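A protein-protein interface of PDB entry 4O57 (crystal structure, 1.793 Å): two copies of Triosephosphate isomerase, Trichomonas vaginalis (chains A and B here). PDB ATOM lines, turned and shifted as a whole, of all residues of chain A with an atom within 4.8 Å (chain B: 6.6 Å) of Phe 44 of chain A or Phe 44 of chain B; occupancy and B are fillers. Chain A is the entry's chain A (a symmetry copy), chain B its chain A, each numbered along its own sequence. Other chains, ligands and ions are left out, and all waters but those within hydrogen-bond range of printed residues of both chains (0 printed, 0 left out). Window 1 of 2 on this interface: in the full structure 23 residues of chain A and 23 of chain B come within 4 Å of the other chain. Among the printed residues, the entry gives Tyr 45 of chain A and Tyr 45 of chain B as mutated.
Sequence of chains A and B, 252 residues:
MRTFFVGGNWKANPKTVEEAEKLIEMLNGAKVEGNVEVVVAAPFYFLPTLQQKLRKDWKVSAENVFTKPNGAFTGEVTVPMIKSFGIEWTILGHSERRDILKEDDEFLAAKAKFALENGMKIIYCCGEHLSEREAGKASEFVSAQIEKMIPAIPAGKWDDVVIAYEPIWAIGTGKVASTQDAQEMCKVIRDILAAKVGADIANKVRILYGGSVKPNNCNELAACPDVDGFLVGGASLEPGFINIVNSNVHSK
Printed residues of chain B within 4 Å of Phe 44 of chain A: Phe 44, Tyr 45 and Gly 75. Of the printed residues of chain A, Phe 44 of chain B touches Phe 44 (3.7 Å), Tyr 45 (3.99 Å) and Gly 75 (3.4 Å). Printed residues of chain B within 4 Å of Tyr 45 of chain A: Phe 44, Leu 47 and Pro 48. Of the printed residues of chain A, Arg 97 of chain B touches Gly 75. The nearest printed residue of chain A that does not touch Leu 47 of chain B is Pro 48 of chain A (6.8 Å).
The side-chain amide nitrogen of Asn 64 of chain B sits close to the guanidinium group of Arg 97 of chain B (3.3 Å).
Of the 18 printed residues of chain B, 7 touch a printed residue of chain A. Of the 11 printed residues of chain A, 5 touch a printed residue of chain B. Printed residues of chain A that touch a printed residue of chain B: Phe 44, Tyr 45, Leu 47, Pro 48 and Gly 75. Hydrophobic or aromatic side chains of chain A that line the printed part of chain B: Phe 44, Tyr 45, Leu 47 and Pro 48.
The side-chain carboxylate of Glu 63 of chain B is in hydrogen-bond range of the backbone NH of Gly 75 of chain A.
Phe 44 of chain A touches Tyr 45 of chain B, and with the chains exchanged Tyr 45 of chain A touches Phe 44 of chain B. Phe 44 of chain A touches Gly 75 of chain B, and with the chains exchanged Gly 75 of chain A touches Phe 44 of chain B. Tyr 45 of chain A touches Leu 47 of chain B, and with the chains exchanged Leu 47 of chain A touches Tyr 45 of chain B. Tyr 45 of chain A touches Pro 48 of chain B, and with the chains exchanged Pro 48 of chain A touches Tyr 45 of chain B.
Phe 44 of chain B touches Phe 44 of chain A. O of Phe 44 of chain A touches CA of Tyr 45 of chain B, at 3.99 Å. Phe 44 of chain A touches Gly 75 of chain B (CE2 to O, 3.4 Å). Phe 44 of chain B touches Tyr 45 of chain A. CB of Leu 47 of chain B touches CE2 of Tyr 45 of chain A (3.97 Å). O of Tyr 45 of chain A touches CG of Pro 48 of chain B (3.4 Å). Leu 47 of chain A touches Tyr 45 of chain B. Pro 48 of chain A touches Tyr 45 of chain B (CG to O, 3.4 Å). CE2 of Phe 44 of chain B touches O of Gly 75 of chain A, at 3.4 Å. Gly 75 of chain A touches Arg 97 of chain B (CA to NH1, 3.4 Å).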
ATOM      1  N   ALA A  42      24.761  26.638  -0.175  1.00  0.00           N
ATOM      2  CA  ALA A  42      24.340  25.253  -0.445  1.00  0.00           C
ATOM      3  C   ALA A  42      22.841  25.164  -0.477  1.00  0.00           C
ATOM      4  O   ALA A  42      22.151  26.024   0.043  1.00  0.00           O
ATOM      5  CB  ALA A  42      24.862  24.308   0.608  1.00  0.00           C
ATOM      6  N   PRO A  43      22.321  24.106  -1.091  1.00  0.00           N
ATOM      7  CA  PRO A  43      20.878  23.949  -1.104  1.00  0.00           C
ATOM      8  C   PRO A  43      20.301  23.942   0.309  1.00  0.00           C
ATOM      9  O   PRO A  43      20.953  23.467   1.241  1.00  0.00           O
ATOM     10  CB  PRO A  43      20.701  22.568  -1.715  1.00  0.00           C
ATOM     11  CG  PRO A  43      21.902  22.392  -2.594  1.00  0.00           C
ATOM     12  CD  PRO A  43      23.008  23.066  -1.882  1.00  0.00           C
ATOM     13  N   PHE A  44      19.054  24.365   0.429  1.00  0.00           N
ATOM     14  CA  PHE A  44      18.412  24.452   1.724  1.00  0.00           C
ATOM     15  C   PHE A  44      18.510  23.152   2.511  1.00  0.00           C
ATOM     16  O   PHE A  44      18.827  23.199   3.694  1.00  0.00           O
ATOM     17  CB  PHE A  44      16.943  24.869   1.600  1.00  0.00           C
ATOM     18  CG  PHE A  44      16.726  26.204   0.880  1.00  0.00           C
ATOM     19  CD1 PHE A  44      17.149  27.398   1.454  1.00  0.00           C
ATOM     20  CD2 PHE A  44      16.071  26.249  -0.356  1.00  0.00           C
ATOM     21  CE1 PHE A  44      16.941  28.616   0.807  1.00  0.00           C
ATOM     22  CE2 PHE A  44      15.872  27.467  -1.013  1.00  0.00           C
ATOM     23  CZ  PHE A  44      16.316  28.644  -0.430  1.00  0.00           C
ATOM     24  N   TYR A  45      18.241  22.006   1.863  1.00  0.00           N
ATOM     25  CA  TYR A  45      18.176  20.718   2.543  1.00  0.00           C
ATOM     26  C   TYR A  45      19.493  20.378   3.230  1.00  0.00           C
ATOM     27  O   TYR A  45      19.516  19.644   4.235  1.00  0.00           O
ATOM     28  CB  TYR A  45      17.788  19.622   1.532  1.00  0.00           C
ATOM     29  CG  TYR A  45      17.680  18.232   2.110  1.00  0.00           C
ATOM     30  CD1 TYR A  45      18.803  17.409   2.203  1.00  0.00           C
ATOM     31  CD2 TYR A  45      16.465  17.735   2.567  1.00  0.00           C
ATOM     32  CE1 TYR A  45      18.715  16.132   2.741  1.00  0.00           C
ATOM     33  CE2 TYR A  45      16.369  16.456   3.100  1.00  0.00           C
ATOM     34  CZ  TYR A  45      17.502  15.658   3.180  1.00  0.00           C
ATOM     35  OH  TYR A  45      17.420  14.393   3.725  1.00  0.00           O
ATOM     36  N   PHE A  46      20.585  20.892   2.687  1.00  0.00           N
ATOM     37  CA  PHE A  46      21.931  20.608   3.192  1.00  0.00           C
ATOM     38  C   PHE A  46      22.444  21.616   4.214  1.00  0.00           C
ATOM     39  O   PHE A  46      23.501  21.388   4.812  1.00  0.00           O
ATOM     40  CB  PHE A  46      22.965  20.595   2.065  1.00  0.00           C
ATOM     41  CG  PHE A  46      22.831  19.460   1.087  1.00  0.00           C
ATOM     42  CD1 PHE A  46      22.379  18.209   1.465  1.00  0.00           C
ATOM     43  CD2 PHE A  46      23.174  19.663  -0.234  1.00  0.00           C
ATOM     44  CE1 PHE A  46      22.275  17.175   0.531  1.00  0.00           C
ATOM     45  CE2 PHE A  46      23.069  18.645  -1.153  1.00  0.00           C
ATOM     46  CZ  PHE A  46      22.618  17.407  -0.777  1.00  0.00           C
ATOM     47  N   LEU A  47      21.799  22.776   4.360  1.00  0.00           N
ATOM     48  CA  LEU A  47      22.335  23.798   5.253  1.00  0.00           C
ATOM     49  C   LEU A  47      22.499  23.281   6.677  1.00  0.00           C
ATOM     50  O   LEU A  47      23.497  23.602   7.311  1.00  0.00           O
ATOM     51  CB  LEU A  47      21.480  25.070   5.241  1.00  0.00           C
ATOM     52  CG  LEU A  47      21.531  25.818   3.886  1.00  0.00           C
ATOM     53  CD1 LEU A  47      20.584  27.032   3.837  1.00  0.00           C
ATOM     54  CD2 LEU A  47      22.905  26.235   3.519  1.00  0.00           C
ATOM     55  N   PRO A  48      21.552  22.459   7.175  1.00  0.00           N
ATOM     56  CA  PRO A  48      21.775  21.989   8.559  1.00  0.00           C
ATOM     57  C   PRO A  48      23.095  21.199   8.719  1.00  0.00           C
ATOM     58  O   PRO A  48      23.869  21.401   9.668  1.00  0.00           O
ATOM     59  CB  PRO A  48      20.552  21.121   8.833  1.00  0.00           C
ATOM     60  CG  PRO A  48      19.470  21.714   7.963  1.00  0.00           C
ATOM     61  CD  PRO A  48      20.171  22.199   6.719  1.00  0.00           C
ATOM     62  N   ALA A  62      22.706  30.833   2.469  1.00  0.00           N
ATOM     63  CA  ALA A  62      21.602  30.443   1.644  1.00  0.00           C
ATOM     64  C   ALA A  62      21.886  30.893   0.195  1.00  0.00           C
ATOM     65  O   ALA A  62      22.665  31.837  -0.022  1.00  0.00           O
ATOM     66  CB  ALA A  62      20.328  31.047   2.155  1.00  0.00           C
ATOM     67  N   ASN A  64      19.409  31.826  -1.679  1.00  0.00           N
ATOM     68  CA  ASN A  64      18.297  32.731  -1.911  1.00  0.00           C
ATOM     69  C   ASN A  64      17.452  32.739  -0.623  1.00  0.00           C
ATOM     70  O   ASN A  64      17.624  31.865   0.224  1.00  0.00           O
ATOM     71  CB  ASN A  64      17.427  32.277  -3.078  1.00  0.00           C
ATOM     72  CG  ASN A  64      16.274  33.220  -3.325  1.00  0.00           C
ATOM     73  OD1 ASN A  64      16.449  34.444  -3.284  1.00  0.00           O
ATOM     74  ND2 ASN A  64      15.075  32.669  -3.523  1.00  0.00           N
ATOM     75  N   GLY A  75       6.299  26.203  -0.296  1.00  0.00           N
ATOM     76  CA  GLY A  75       7.498  25.920  -1.068  1.00  0.00           C
ATOM     77  C   GLY A  75       8.633  26.889  -0.803  1.00  0.00           C
ATOM     78  O   GLY A  75       9.736  26.688  -1.292  1.00  0.00           O
ATOM     79  N   VAL A  77      11.101  29.648   1.715  1.00  0.00           N
ATOM     80  CA  VAL A  77      11.949  29.643   2.924  1.00  0.00           C
ATOM     81  C   VAL A  77      12.289  31.082   3.364  1.00  0.00           C
ATOM     82  O   VAL A  77      12.501  31.931   2.522  1.00  0.00           O
ATOM     83  CB  VAL A  77      13.282  28.906   2.623  1.00  0.00           C
ATOM     84  CG1 VAL A  77      14.277  29.005   3.801  1.00  0.00           C
ATOM     85  CG2 VAL A  77      12.997  27.462   2.256  1.00  0.00           C
ATOM     86  N   ALA B  42       6.851  20.016   4.818  1.00  0.00           N
ATOM     87  CA  ALA B  42       7.567  21.013   5.631  1.00  0.00           C
ATOM     88  C   ALA B  42       8.595  21.721   4.797  1.00  0.00           C
ATOM     89  O   ALA B  42       9.003  21.232   3.757  1.00  0.00           O
ATOM     90  CB  ALA B  42       8.255  20.367   6.808  1.00  0.00           C
ATOM     91  N   PRO B  43       9.030  22.891   5.254  1.00  0.00           N
ATOM     92  CA  PRO B  43      10.062  23.589   4.509  1.00  0.00           C
ATOM     93  C   PRO B  43      11.303  22.722   4.321  1.00  0.00           C
ATOM     94  O   PRO B  43      11.630  21.911   5.190  1.00  0.00           O
ATOM     95  CB  PRO B  43      10.407  24.749   5.428  1.00  0.00           C
ATOM     96  CG  PRO B  43       9.144  25.005   6.195  1.00  0.00           C
ATOM     97  CD  PRO B  43       8.538  23.674   6.404  1.00  0.00           C
ATOM     98  N   PHE B  44      12.034  22.978   3.249  1.00  0.00           N
ATOM     99  CA  PHE B  44      13.208  22.191   2.935  1.00  0.00           C
ATOM    100  C   PHE B  44      14.173  22.092   4.108  1.00  0.00           C
ATOM    101  O   PHE B  44      14.652  20.999   4.389  1.00  0.00           O
ATOM    102  CB  PHE B  44      13.944  22.739   1.707  1.00  0.00           C
ATOM    103  CG  PHE B  44      13.083  22.820   0.442  1.00  0.00           C
ATOM    104  CD1 PHE B  44      12.632  21.665  -0.186  1.00  0.00           C
ATOM    105  CD2 PHE B  44      12.761  24.061  -0.122  1.00  0.00           C
ATOM    106  CE1 PHE B  44      11.859  21.737  -1.345  1.00  0.00           C
ATOM    107  CE2 PHE B  44      11.977  24.136  -1.278  1.00  0.00           C
ATOM    108  CZ  PHE B  44      11.524  22.971  -1.877  1.00  0.00           C
ATOM    109  N   TYR B  45      14.457  23.219   4.782  1.00  0.00           N
ATOM    110  CA  TYR B  45      15.463  23.269   5.837  1.00  0.00           C
ATOM    111  C   TYR B  45      15.136  22.308   6.972  1.00  0.00           C
ATOM    112  O   TYR B  45      16.040  21.823   7.676  1.00  0.00           O
ATOM    113  CB  TYR B  45      15.587  24.713   6.360  1.00  0.00           C
ATOM    114  CG  TYR B  45      16.605  24.907   7.458  1.00  0.00           C
ATOM    115  CD1 TYR B  45      16.257  24.709   8.795  1.00  0.00           C
ATOM    116  CD2 TYR B  45      17.911  25.283   7.170  1.00  0.00           C
ATOM    117  CE1 TYR B  45      17.189  24.877   9.811  1.00  0.00           C
ATOM    118  CE2 TYR B  45      18.846  25.460   8.182  1.00  0.00           C
ATOM    119  CZ  TYR B  45      18.474  25.257   9.505  1.00  0.00           C
ATOM    120  OH  TYR B  45      19.400  25.411  10.514  1.00  0.00           O
ATOM    121  N   PHE B  46      13.853  22.045   7.164  1.00  0.00           N
ATOM    122  CA  PHE B  46      13.372  21.191   8.253  1.00  0.00           C
ATOM    123  C   PHE B  46      13.209  19.723   7.875  1.00  0.00           C
ATOM    124  O   PHE B  46      12.955  18.896   8.756  1.00  0.00           O
ATOM    125  CB  PHE B  46      12.004  21.644   8.763  1.00  0.00           C
ATOM    126  CG  PHE B  46      11.993  22.970   9.474  1.00  0.00           C
ATOM    127  CD1 PHE B  46      13.062  23.409  10.233  1.00  0.00           C
ATOM    128  CD2 PHE B  46      10.880  23.780   9.376  1.00  0.00           C
ATOM    129  CE1 PHE B  46      13.014  24.643  10.888  1.00  0.00           C
ATOM    130  CE2 PHE B  46      10.835  24.995  10.019  1.00  0.00           C
ATOM    131  CZ  PHE B  46      11.896  25.429  10.768  1.00  0.00           C
ATOM    132  N   LEU B  47      13.233  19.380   6.585  1.00  0.00           N
ATOM    133  CA  LEU B  47      12.970  17.998   6.196  1.00  0.00           C
ATOM    134  C   LEU B  47      13.939  17.026   6.858  1.00  0.00           C
ATOM    135  O   LEU B  47      13.510  15.956   7.274  1.00  0.00           O
ATOM    136  CB  LEU B  47      12.993  17.822   4.673  1.00  0.00           C
ATOM    137  CG  LEU B  47      11.822  18.546   3.965  1.00  0.00           C
ATOM    138  CD1 LEU B  47      11.909  18.463   2.430  1.00  0.00           C
ATOM    139  CD2 LEU B  47      10.497  18.066   4.422  1.00  0.00           C
ATOM    140  N   PRO B  48      15.229  17.396   6.993  1.00  0.00           N
ATOM    141  CA  PRO B  48      16.113  16.410   7.649  1.00  0.00           C
ATOM    142  C   PRO B  48      15.660  16.061   9.086  1.00  0.00           C
ATOM    143  O   PRO B  48      15.623  14.889   9.496  1.00  0.00           O
ATOM    144  CB  PRO B  48      17.474  17.096   7.630  1.00  0.00           C
ATOM    145  CG  PRO B  48      17.425  17.992   6.415  1.00  0.00           C
ATOM    146  CD  PRO B  48      15.997  18.463   6.318  1.00  0.00           C
ATOM    147  N   ALA B  62       8.024  16.981   0.549  1.00  0.00           N
ATOM    148  CA  ALA B  62       8.439  18.277   0.104  1.00  0.00           C
ATOM    149  C   ALA B  62       7.182  19.106  -0.239  1.00  0.00           C
ATOM    150  O   ALA B  62       6.122  18.532  -0.540  1.00  0.00           O
ATOM    151  CB  ALA B  62       9.345  18.157  -1.085  1.00  0.00           C
ATOM    152  N   GLU B  63       7.294  20.432  -0.155  1.00  0.00           N
ATOM    153  CA  GLU B  63       6.188  21.324  -0.535  1.00  0.00           C
ATOM    154  C   GLU B  63       6.215  21.636  -2.029  1.00  0.00           C
ATOM    155  O   GLU B  63       5.248  22.190  -2.603  1.00  0.00           O
ATOM    156  CB  GLU B  63       6.216  22.619   0.318  1.00  0.00           C
ATOM    157  CG  GLU B  63       6.021  22.350   1.805  1.00  0.00           C
ATOM    158  CD  GLU B  63       6.032  23.597   2.688  1.00  0.00           C
ATOM    159  OE1 GLU B  63       5.962  24.723   2.168  1.00  0.00           O
ATOM    160  OE2 GLU B  63       6.134  23.409   3.925  1.00  0.00           O
ATOM    161  N   ASN B  64       7.322  21.247  -2.671  1.00  0.00           N
ATOM    162  CA  ASN B  64       7.544  21.514  -4.082  1.00  0.00           C
ATOM    163  C   ASN B  64       8.883  20.854  -4.456  1.00  0.00           C
ATOM    164  O   ASN B  64       9.653  20.490  -3.569  1.00  0.00           O
ATOM    165  CB  ASN B  64       7.622  23.009  -4.372  1.00  0.00           C
ATOM    166  CG  ASN B  64       7.845  23.289  -5.839  1.00  0.00           C
ATOM    167  OD1 ASN B  64       7.226  22.648  -6.698  1.00  0.00           O
ATOM    168  ND2 ASN B  64       8.770  24.201  -6.146  1.00  0.00           N
ATOM    169  N   VAL B  65       9.146  20.659  -5.738  1.00  0.00           N
ATOM    170  CA  VAL B  65      10.478  20.215  -6.179  1.00  0.00           C
ATOM    171  C   VAL B  65      10.798  20.815  -7.505  1.00  0.00           C
ATOM    172  O   VAL B  65       9.889  21.204  -8.228  1.00  0.00           O
ATOM    173  CB  VAL B  65      10.553  18.687  -6.338  1.00  0.00           C
ATOM    174  CG1 VAL B  65      10.332  18.001  -5.023  1.00  0.00           C
ATOM    175  CG2 VAL B  65       9.532  18.230  -7.334  1.00  0.00           C
ATOM    176  N   PHE B  66      12.089  20.915  -7.834  1.00  0.00           N
ATOM    177  CA  PHE B  66      12.515  21.494  -9.107  1.00  0.00           C
ATOM    178  C   PHE B  66      12.491  20.473 -10.247  1.00  0.00           C
ATOM    179  O   PHE B  66      12.625  19.272 -10.008  1.00  0.00           O
ATOM    180  CB  PHE B  66      13.925  22.086  -8.983  1.00  0.00           C
ATOM    181  CG  PHE B  66      14.462  22.630 -10.277  1.00  0.00           C
ATOM    182  CD1 PHE B  66      14.038  23.853 -10.761  1.00  0.00           C
ATOM    183  CD2 PHE B  66      15.386  21.905 -11.012  1.00  0.00           C
ATOM    184  CE1 PHE B  66      14.537  24.349 -11.958  1.00  0.00           C
ATOM    185  CE2 PHE B  66      15.883  22.391 -12.203  1.00  0.00           C
ATOM    186  CZ  PHE B  66      15.457  23.611 -12.679  1.00  0.00           C
ATOM    187  N   GLY B  75      19.399  28.230  -5.958  1.00  0.00           N
ATOM    188  CA  GLY B  75      18.248  28.448  -5.098  1.00  0.00           C
ATOM    189  C   GLY B  75      17.227  27.329  -5.152  1.00  0.00           C
ATOM    190  O   GLY B  75      16.276  27.331  -4.383  1.00  0.00           O
ATOM    191  N   GLU B  76      17.443  26.370  -6.048  1.00  0.00           N
ATOM    192  CA  GLU B  76      16.461  25.329  -6.333  1.00  0.00           C
ATOM    193  C   GLU B  76      16.896  23.937  -5.834  1.00  0.00           C
ATOM    194  O   GLU B  76      18.084  23.654  -5.725  1.00  0.00           O
ATOM    195  CB  GLU B  76      16.198  25.283  -7.838  1.00  0.00           C
ATOM    196  N   VAL B  77      15.895  23.076  -5.577  1.00  0.00           N
ATOM    197  CA  VAL B  77      16.054  21.758  -4.932  1.00  0.00           C
ATOM    198  C   VAL B  77      15.472  20.638  -5.818  1.00  0.00           C
ATOM    199  O   VAL B  77      14.458  20.844  -6.454  1.00  0.00           O
ATOM    200  CB  VAL B  77      15.292  21.744  -3.580  1.00  0.00           C
ATOM    201  CG1 VAL B  77      15.288  20.342  -2.931  1.00  0.00           C
ATOM    202  CG2 VAL B  77      15.883  22.786  -2.648  1.00  0.00           C
ATOM    203  N   THR B  78      16.069  19.446  -5.819  1.00  0.00           N
ATOM    204  CA  THR B  78      15.792  18.475  -6.878  1.00  0.00           C
ATOM    205  C   THR B  78      15.378  17.110  -6.358  1.00  0.00           C
ATOM    206  O   THR B  78      15.504  16.798  -5.177  1.00  0.00           O
ATOM    207  CB  THR B  78      17.010  18.289  -7.784  1.00  0.00           C
ATOM    208  OG1 THR B  78      17.967  17.462  -7.114  1.00  0.00           O
ATOM    209  CG2 THR B  78      17.640  19.650  -8.122  1.00  0.00           C
ATOM    210  N   ILE B  82      16.070  14.931  -2.511  1.00  0.00           N
ATOM    211  CA  ILE B  82      15.027  14.572  -1.582  1.00  0.00           C
ATOM    212  C   ILE B  82      14.876  13.062  -1.641  1.00  0.00           C
ATOM    213  O   ILE B  82      14.824  12.425  -0.598  1.00  0.00           O
ATOM    214  CB  ILE B  82      13.704  15.315  -1.850  1.00  0.00           C
ATOM    215  CG1 ILE B  82      13.190  15.038  -3.260  1.00  0.00           C
ATOM    216  CG2 ILE B  82      13.917  16.823  -1.636  1.00  0.00           C
ATOM    217  CD1 ILE B  82      11.809  15.570  -3.487  1.00  0.00           C
ATOM    218  N   ARG B  97       1.601  28.566  -5.421  1.00  0.00           N
ATOM    219  CA  ARG B  97       2.691  28.522  -6.403  1.00  0.00           C
ATOM    220  C   ARG B  97       2.188  28.768  -7.828  1.00  0.00           C
ATOM    221  O   ARG B  97       2.837  29.482  -8.611  1.00  0.00           O
ATOM    222  CB  ARG B  97       3.454  27.198  -6.326  1.00  0.00           C
ATOM    223  CG  ARG B  97       4.074  26.949  -4.946  1.00  0.00           C
ATOM    224  CD  ARG B  97       5.142  25.852  -4.984  1.00  0.00           C
ATOM    225  NE  ARG B  97       6.313  26.307  -5.732  1.00  0.00           N
ATOM    226  CZ  ARG B  97       7.240  27.134  -5.259  1.00  0.00           C
ATOM    227  NH1 ARG B  97       7.161  27.593  -4.020  1.00  0.00           N
ATOM    228  NH2 ARG B  97       8.258  27.497  -6.033  1.00  0.00           N
